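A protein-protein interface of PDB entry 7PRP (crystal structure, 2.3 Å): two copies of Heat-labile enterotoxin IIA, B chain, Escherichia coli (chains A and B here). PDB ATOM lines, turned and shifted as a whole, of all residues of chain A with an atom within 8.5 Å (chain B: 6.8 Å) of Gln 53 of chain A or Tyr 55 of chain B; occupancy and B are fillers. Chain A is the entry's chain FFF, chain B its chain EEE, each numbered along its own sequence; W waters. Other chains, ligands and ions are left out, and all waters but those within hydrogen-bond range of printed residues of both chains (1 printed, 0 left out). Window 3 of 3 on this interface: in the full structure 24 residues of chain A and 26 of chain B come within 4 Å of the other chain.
Water W1 lies within hydrogen-bond range of the backbone carbonyl oxygen (O) of Ile 49 of chain A and the side-chain hydroxyl (OH) of Tyr 59 of chain B.
OH of Tyr 55 of chain B sits at hydrogen-bond distance from N of Gly 52 of chain A (3.1 Å). The side-chain amino group (NZ) of Lys 35 of chain A is in salt-bridge range of the side-chain carboxylate (OD1) of Asp 57 of chain B (2.6 Å).
Of the 8 printed residues of chain B, 4 touch a printed residue of chain A. Printed residues of chain B that touch a printed residue of chain A: Tyr 55, Pro 56, Asp 57 and Tyr 59. Hydrophobic or aromatic side chains of chain B that line the printed part of chain A: Tyr 55, Pro 56 and Tyr 59. Of the 15 printed residues of chain A, 5 touch a printed residue of chain B. Printed residues of chain A that touch a printed residue of chain B: Lys 35, Gly 51, Gly 52, Gln 53 and Arg 65.
Gly 52 of chain A touches Tyr 55 of chain B, but with the chains exchanged Tyr 55 of chain A does not touch Gly 52 of chain B (17.0 Å). Gln 53 of chain A touches Tyr 55 of chain B, but with the chains exchanged Tyr 55 of chain A does not touch Gln 53 of chain B (14.8 Å).
Gln 53 of chain A touches just one residue of chain B: Tyr 55. Tyr 55 of chain B touches three residues of chain A. Printed residues of chain A within 4 Å of Tyr 59 of chain B: Gly 51 and Arg 65. Printed residues of chain B within 4 Å of Gly 51 of chain A: Tyr 55 and Tyr 59. The nearest residue of chain B that does not touch Gln 53 of chain A is Pro 56 of chain B (6.5 Å). The nearest printed residue of chain A that does not touch Tyr 59 of chain B is Pro 50 of chain A (4.7 Å).
The backbone NH of Tyr 55 of chain B sits close to the side-chain amide nitrogen of Asn 58 of chain B (3.5 Å). The side-chain amide oxygen (OD1) of Asn 58 of chain B sits close to the backbone carbonyl oxygen (O) of Pro 56 of chain B. N of Gly 52 of chain A lies within hydrogen-bond range of OG of Ser 61 of chain A, 3.4 Å away. The guanidinium group of Arg 65 of chain A lies within hydrogen-bond range of the side-chain hydroxyl of Ser 61 of chain A, at 3.1 Å.
Pro 56 of chain B touches Lys 35 of chain A. Tyr 55 of chain B touches Gly 51 of chain A. Gly 51 of chain A touches Tyr 59 of chain B. Tyr 55 of chain B touches Gln 53 of chain A (CD1 to OE1, 3.5 Å). Arg 65 of chain A touches Tyr 59 of chain B.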
ATOM      1  N   LYS A  35     -28.481  10.020  30.004  1.00  0.00           N
ATOM      2  CA  LYS A  35     -27.370   9.089  29.729  1.00  0.00           C
ATOM      3  C   LYS A  35     -27.319   8.725  28.246  1.00  0.00           C
ATOM      4  O   LYS A  35     -28.375   8.439  27.682  1.00  0.00           O
ATOM      5  CB  LYS A  35     -27.533   7.823  30.565  1.00  0.00           C
ATOM      6  CG  LYS A  35     -26.900   7.891  31.948  1.00  0.00           C
ATOM      7  CD  LYS A  35     -26.906   6.603  32.746  1.00  0.00           C
ATOM      8  CE  LYS A  35     -26.258   6.883  34.082  1.00  0.00           C
ATOM      9  NZ  LYS A  35     -26.453   5.753  34.997  1.00  0.00           N
ATOM     10  N   PHE A  48     -28.987   9.964  18.553  1.00  0.00           N
ATOM     11  CA  PHE A  48     -28.558   9.132  19.679  1.00  0.00           C
ATOM     12  C   PHE A  48     -28.019   7.815  19.105  1.00  0.00           C
ATOM     13  O   PHE A  48     -28.650   7.227  18.182  1.00  0.00           O
ATOM     14  CB  PHE A  48     -29.747   8.951  20.601  1.00  0.00           C
ATOM     15  CG  PHE A  48     -29.563   7.917  21.686  1.00  0.00           C
ATOM     16  CD1 PHE A  48     -28.978   8.249  22.900  1.00  0.00           C
ATOM     17  CD2 PHE A  48     -30.008   6.615  21.521  1.00  0.00           C
ATOM     18  CE1 PHE A  48     -28.859   7.324  23.918  1.00  0.00           C
ATOM     19  CE2 PHE A  48     -29.878   5.688  22.543  1.00  0.00           C
ATOM     20  CZ  PHE A  48     -29.322   6.054  23.749  1.00  0.00           C
ATOM     21  N   ILE A  49     -26.851   7.407  19.590  1.00  0.00           N
ATOM     22  CA  ILE A  49     -26.257   6.083  19.286  1.00  0.00           C
ATOM     23  C   ILE A  49     -26.575   5.140  20.440  1.00  0.00           C
ATOM     24  O   ILE A  49     -26.070   5.298  21.545  1.00  0.00           O
ATOM     25  CB  ILE A  49     -24.757   6.161  19.052  1.00  0.00           C
ATOM     26  CG1 ILE A  49     -24.391   7.233  18.032  1.00  0.00           C
ATOM     27  CG2 ILE A  49     -24.229   4.778  18.695  1.00  0.00           C
ATOM     28  CD1 ILE A  49     -22.913   7.232  17.665  1.00  0.00           C
ATOM     29  N   PRO A  50     -27.431   4.132  20.226  1.00  0.00           N
ATOM     30  CA  PRO A  50     -27.725   3.160  21.270  1.00  0.00           C
ATOM     31  C   PRO A  50     -26.502   2.327  21.662  1.00  0.00           C
ATOM     32  O   PRO A  50     -25.614   2.111  20.842  1.00  0.00           O
ATOM     33  CB  PRO A  50     -28.777   2.220  20.686  1.00  0.00           C
ATOM     34  CG  PRO A  50     -28.792   2.504  19.204  1.00  0.00           C
ATOM     35  CD  PRO A  50     -28.127   3.855  18.971  1.00  0.00           C
ATOM     36  N   GLY A  51     -26.466   1.952  22.940  1.00  0.00           N
ATOM     37  CA  GLY A  51     -25.460   1.067  23.539  1.00  0.00           C
ATOM     38  C   GLY A  51     -25.873  -0.382  23.388  1.00  0.00           C
ATOM     39  O   GLY A  51     -26.974  -0.658  22.917  1.00  0.00           O
ATOM     40  N   GLY A  52     -25.015  -1.273  23.831  1.00  0.00           N
ATOM     41  CA  GLY A  52     -25.237  -2.716  23.801  1.00  0.00           C
ATOM     42  C   GLY A  52     -24.586  -3.375  24.983  1.00  0.00           C
ATOM     43  O   GLY A  52     -23.404  -3.151  25.195  1.00  0.00           O
ATOM     44  N   GLN A  53     -25.354  -4.155  25.732  1.00  0.00           N
ATOM     45  CA  GLN A  53     -24.837  -4.855  26.926  1.00  0.00           C
ATOM     46  C   GLN A  53     -24.388  -6.270  26.540  1.00  0.00           C
ATOM     47  O   GLN A  53     -23.485  -6.752  27.188  1.00  0.00           O
ATOM     48  CB  GLN A  53     -25.925  -4.845  27.987  1.00  0.00           C
ATOM     49  CG  GLN A  53     -25.425  -5.326  29.338  1.00  0.00           C
ATOM     50  CD  GLN A  53     -26.418  -4.976  30.425  1.00  0.00           C
ATOM     51  OE1 GLN A  53     -27.486  -4.405  30.175  1.00  0.00           O
ATOM     52  NE2 GLN A  53     -26.033  -5.260  31.651  1.00  0.00           N
ATOM     53  N   TYR A  54     -24.969  -6.893  25.513  1.00  0.00           N
ATOM     54  CA  TYR A  54     -24.772  -8.343  25.244  1.00  0.00           C
ATOM     55  C   TYR A  54     -24.191  -8.496  23.847  1.00  0.00           C
ATOM     56  O   TYR A  54     -24.487  -7.659  22.982  1.00  0.00           O
ATOM     57  CB  TYR A  54     -26.091  -9.136  25.400  1.00  0.00           C
ATOM     58  CG  TYR A  54     -26.657  -9.070  26.802  1.00  0.00           C
ATOM     59  CD1 TYR A  54     -26.029  -9.701  27.870  1.00  0.00           C
ATOM     60  CD2 TYR A  54     -27.758  -8.288  27.089  1.00  0.00           C
ATOM     61  CE1 TYR A  54     -26.510  -9.598  29.171  1.00  0.00           C
ATOM     62  CE2 TYR A  54     -28.238  -8.157  28.383  1.00  0.00           C
ATOM     63  CZ  TYR A  54     -27.619  -8.820  29.428  1.00  0.00           C
ATOM     64  OH  TYR A  54     -28.110  -8.670  30.691  1.00  0.00           O
ATOM     65  N   TYR A  55     -23.402  -9.554  23.625  1.00  0.00           N
ATOM     66  CA  TYR A  55     -22.913  -9.909  22.274  1.00  0.00           C
ATOM     67  C   TYR A  55     -24.143 -10.124  21.389  1.00  0.00           C
ATOM     68  O   TYR A  55     -25.059 -10.813  21.807  1.00  0.00           O
ATOM     69  CB  TYR A  55     -21.992 -11.124  22.336  1.00  0.00           C
ATOM     70  CG  TYR A  55     -21.403 -11.534  21.005  1.00  0.00           C
ATOM     71  CD1 TYR A  55     -22.122 -12.284  20.084  1.00  0.00           C
ATOM     72  CD2 TYR A  55     -20.137 -11.099  20.637  1.00  0.00           C
ATOM     73  CE1 TYR A  55     -21.581 -12.636  18.852  1.00  0.00           C
ATOM     74  CE2 TYR A  55     -19.576 -11.438  19.409  1.00  0.00           C
ATOM     75  CZ  TYR A  55     -20.298 -12.214  18.515  1.00  0.00           C
ATOM     76  OH  TYR A  55     -19.730 -12.545  17.319  1.00  0.00           O
ATOM     77  N   PRO A  56     -24.220  -9.631  20.127  1.00  0.00           N
ATOM     78  CA  PRO A  56     -23.148  -8.866  19.485  1.00  0.00           C
ATOM     79  C   PRO A  56     -23.239  -7.344  19.581  1.00  0.00           C
ATOM     80  O   PRO A  56     -22.312  -6.693  19.205  1.00  0.00           O
ATOM     81  CB  PRO A  56     -23.271  -9.302  18.020  1.00  0.00           C
ATOM     82  CG  PRO A  56     -24.774  -9.492  17.849  1.00  0.00           C
ATOM     83  CD  PRO A  56     -25.313  -9.959  19.201  1.00  0.00           C
ATOM     84  N   ASP A  57     -24.336  -6.812  20.123  1.00  0.00           N
ATOM     85  CA  ASP A  57     -24.594  -5.349  20.161  1.00  0.00           C
ATOM     86  C   ASP A  57     -23.475  -4.635  20.929  1.00  0.00           C
ATOM     87  O   ASP A  57     -23.188  -3.488  20.620  1.00  0.00           O
ATOM     88  CB  ASP A  57     -25.974  -5.080  20.741  1.00  0.00           C
ATOM     89  CG  ASP A  57     -27.138  -5.487  19.827  1.00  0.00           C
ATOM     90  OD1 ASP A  57     -27.081  -6.591  19.220  1.00  0.00           O
ATOM     91  OD2 ASP A  57     -28.093  -4.707  19.728  1.00  0.00           O
ATOM     92  N   ASN A  58     -22.841  -5.288  21.891  1.00  0.00           N
ATOM     93  CA  ASN A  58     -21.773  -4.645  22.695  1.00  0.00           C
ATOM     94  C   ASN A  58     -20.632  -4.201  21.770  1.00  0.00           C
ATOM     95  O   ASN A  58     -20.275  -2.997  21.861  1.00  0.00           O
ATOM     96  CB  ASN A  58     -21.298  -5.527  23.853  1.00  0.00           C
ATOM     97  CG  ASN A  58     -20.866  -6.939  23.445  1.00  0.00           C
ATOM     98  OD1 ASN A  58     -20.809  -7.340  22.262  1.00  0.00           O
ATOM     99  ND2 ASN A  58     -20.550  -7.711  24.462  1.00  0.00           N
ATOM    100  N   TYR A  59     -20.098  -5.089  20.906  1.00  0.00           N
ATOM    101  CA  TYR A  59     -18.938  -4.731  20.051  1.00  0.00           C
ATOM    102  C   TYR A  59     -19.472  -3.862  18.921  1.00  0.00           C
ATOM    103  O   TYR A  59     -18.790  -2.892  18.572  1.00  0.00           O
ATOM    104  CB  TYR A  59     -18.099  -5.949  19.599  1.00  0.00           C
ATOM    105  CG  TYR A  59     -18.577  -6.711  18.385  1.00  0.00           C
ATOM    106  CD1 TYR A  59     -18.290  -6.287  17.087  1.00  0.00           C
ATOM    107  CD2 TYR A  59     -19.303  -7.873  18.537  1.00  0.00           C
ATOM    108  CE1 TYR A  59     -18.740  -6.998  15.985  1.00  0.00           C
ATOM    109  CE2 TYR A  59     -19.753  -8.592  17.440  1.00  0.00           C
ATOM    110  CZ  TYR A  59     -19.482  -8.161  16.158  1.00  0.00           C
ATOM    111  OH  TYR A  59     -19.950  -8.921  15.109  1.00  0.00           O
ATOM    112  N   SER A  61     -21.986  -1.661  18.811  1.00  0.00           N
ATOM    113  CA  SER A  61     -22.253  -0.284  19.279  1.00  0.00           C
ATOM    114  C   SER A  61     -20.896   0.396  19.524  1.00  0.00           C
ATOM    115  O   SER A  61     -20.753   1.552  19.162  1.00  0.00           O
ATOM    116  CB  SER A  61     -23.140  -0.273  20.507  1.00  0.00           C
ATOM    117  OG  SER A  61     -22.451  -0.708  21.671  1.00  0.00           O
ATOM    118  N   ARG A  65     -19.541   3.899  17.770  1.00  0.00           N
ATOM    119  CA  ARG A  65     -18.948   5.048  18.517  1.00  0.00           C
ATOM    120  C   ARG A  65     -17.561   5.396  17.940  1.00  0.00           C
ATOM    121  O   ARG A  65     -17.283   6.609  17.731  1.00  0.00           O
ATOM    122  CB  ARG A  65     -18.899   4.731  20.023  1.00  0.00           C
ATOM    123  CG  ARG A  65     -20.273   4.524  20.618  1.00  0.00           C
ATOM    124  CD  ARG A  65     -20.224   4.454  22.111  1.00  0.00           C
ATOM    125  NE  ARG A  65     -19.419   3.356  22.644  1.00  0.00           N
ATOM    126  CZ  ARG A  65     -19.897   2.160  22.992  1.00  0.00           C
ATOM    127  NH1 ARG A  65     -19.079   1.248  23.493  1.00  0.00           N
ATOM    128  NH2 ARG A  65     -21.187   1.891  22.868  1.00  0.00           N
ATOM    129  N   GLY B  52     -16.963   4.161  35.838  1.00  0.00           N
ATOM    130  CA  GLY B  52     -18.202   3.366  35.822  1.00  0.00           C
ATOM    131  C   GLY B  52     -17.848   1.898  35.825  1.00  0.00           C
ATOM    132  O   GLY B  52     -17.046   1.464  34.956  1.00  0.00           O
ATOM    133  N   GLN B  53     -18.389   1.155  36.786  1.00  0.00           N
ATOM    134  CA  GLN B  53     -18.128  -0.292  36.908  1.00  0.00           C
ATOM    135  C   GLN B  53     -19.222  -1.052  36.158  1.00  0.00           C
ATOM    136  O   GLN B  53     -18.904  -2.139  35.658  1.00  0.00           O
ATOM    137  CB  GLN B  53     -18.049  -0.661  38.379  1.00  0.00           C
ATOM    138  CG  GLN B  53     -17.602  -2.090  38.597  1.00  0.00           C
ATOM    139  CD  GLN B  53     -17.195  -2.345  40.029  1.00  0.00           C
ATOM    140  OE1 GLN B  53     -17.327  -1.482  40.916  1.00  0.00           O
ATOM    141  NE2 GLN B  53     -16.666  -3.550  40.234  1.00  0.00           N
ATOM    142  N   TYR B  54     -20.441  -0.505  36.039  1.00  0.00           N
ATOM    143  CA  TYR B  54     -21.598  -1.288  35.546  1.00  0.00           C
ATOM    144  C   TYR B  54     -22.146  -0.637  34.291  1.00  0.00           C
ATOM    145  O   TYR B  54     -22.069   0.584  34.160  1.00  0.00           O
ATOM    146  CB  TYR B  54     -22.674  -1.422  36.645  1.00  0.00           C
ATOM    147  CG  TYR B  54     -22.186  -2.186  37.856  1.00  0.00           C
ATOM    148  CD1 TYR B  54     -21.909  -3.550  37.796  1.00  0.00           C
ATOM    149  CD2 TYR B  54     -21.907  -1.523  39.039  1.00  0.00           C
ATOM    150  CE1 TYR B  54     -21.401  -4.235  38.892  1.00  0.00           C
ATOM    151  CE2 TYR B  54     -21.397  -2.197  40.143  1.00  0.00           C
ATOM    152  CZ  TYR B  54     -21.160  -3.559  40.077  1.00  0.00           C
ATOM    153  OH  TYR B  54     -20.622  -4.191  41.160  1.00  0.00           O
ATOM    154  N   TYR B  55     -22.713  -1.444  33.401  1.00  0.00           N
ATOM    155  CA  TYR B  55     -23.436  -0.949  32.213  1.00  0.00           C
ATOM    156  C   TYR B  55     -24.566  -0.047  32.694  1.00  0.00           C
ATOM    157  O   TYR B  55     -25.283  -0.442  33.595  1.00  0.00           O
ATOM    158  CB  TYR B  55     -23.901  -2.124  31.357  1.00  0.00           C
ATOM    159  CG  TYR B  55     -24.565  -1.710  30.064  1.00  0.00           C
ATOM    160  CD1 TYR B  55     -25.891  -1.322  30.041  1.00  0.00           C
ATOM    161  CD2 TYR B  55     -23.844  -1.632  28.879  1.00  0.00           C
ATOM    162  CE1 TYR B  55     -26.504  -0.936  28.851  1.00  0.00           C
ATOM    163  CE2 TYR B  55     -24.434  -1.216  27.686  1.00  0.00           C
ATOM    164  CZ  TYR B  55     -25.772  -0.879  27.670  1.00  0.00           C
ATOM    165  OH  TYR B  55     -26.376  -0.492  26.517  1.00  0.00           O
ATOM    166  N   PRO B  56     -24.825   1.155  32.104  1.00  0.00           N
ATOM    167  CA  PRO B  56     -24.082   1.683  30.955  1.00  0.00           C
ATOM    168  C   PRO B  56     -22.914   2.635  31.281  1.00  0.00           C
ATOM    169  O   PRO B  56     -22.188   2.974  30.385  1.00  0.00           O
ATOM    170  CB  PRO B  56     -25.187   2.424  30.200  1.00  0.00           C
ATOM    171  CG  PRO B  56     -26.037   3.006  31.325  1.00  0.00           C
ATOM    172  CD  PRO B  56     -25.994   1.982  32.439  1.00  0.00           C
ATOM    173  N   ASP B  57     -22.728   3.007  32.543  1.00  0.00           N
ATOM    174  CA  ASP B  57     -21.706   4.013  32.946  1.00  0.00           C
ATOM    175  C   ASP B  57     -20.305   3.520  32.546  1.00  0.00           C
ATOM    176  O   ASP B  57     -19.448   4.340  32.291  1.00  0.00           O
ATOM    177  CB  ASP B  57     -21.795   4.295  34.448  1.00  0.00           C
ATOM    178  CG  ASP B  57     -23.062   5.032  34.895  1.00  0.00           C
ATOM    179  OD1 ASP B  57     -24.167   4.627  34.467  1.00  0.00           O
ATOM    180  OD2 ASP B  57     -22.940   6.029  35.661  1.00  0.00           O
ATOM    181  N   ASN B  58     -20.075   2.210  32.466  1.00  0.00           N
ATOM    182  CA  ASN B  58     -18.745   1.667  32.107  1.00  0.00           C
ATOM    183  C   ASN B  58     -18.331   2.164  30.717  1.00  0.00           C
ATOM    184  O   ASN B  58     -17.224   2.728  30.636  1.00  0.00           O
ATOM    185  CB  ASN B  58     -18.670   0.145  32.226  1.00  0.00           C
ATOM    186  CG  ASN B  58     -19.752  -0.616  31.486  1.00  0.00           C
ATOM    187  OD1 ASN B  58     -20.574  -0.082  30.753  1.00  0.00           O
ATOM    188  ND2 ASN B  58     -19.737  -1.912  31.678  1.00  0.00           N
ATOM    189  N   TYR B  59     -19.188   2.008  29.693  1.00  0.00           N
ATOM    190  CA  TYR B  59     -18.827   2.405  28.312  1.00  0.00           C
ATOM    191  C   TYR B  59     -18.917   3.923  28.242  1.00  0.00           C
ATOM    192  O   TYR B  59     -18.049   4.519  27.600  1.00  0.00           O
ATOM    193  CB  TYR B  59     -19.599   1.633  27.221  1.00  0.00           C
ATOM    194  CG  TYR B  59     -20.962   2.158  26.859  1.00  0.00           C
ATOM    195  CD1 TYR B  59     -21.136   3.213  25.972  1.00  0.00           C
ATOM    196  CD2 TYR B  59     -22.093   1.582  27.388  1.00  0.00           C
ATOM    197  CE1 TYR B  59     -22.396   3.686  25.642  1.00  0.00           C
ATOM    198  CE2 TYR B  59     -23.367   2.026  27.051  1.00  0.00           C
ATOM    199  CZ  TYR B  59     -23.519   3.100  26.195  1.00  0.00           C
ATOM    200  OH  TYR B  59     -24.783   3.542  25.890  1.00  0.00           O
HETATM  201  O   HOH W   1     -25.485   5.694  24.242  1.00  0.00           O
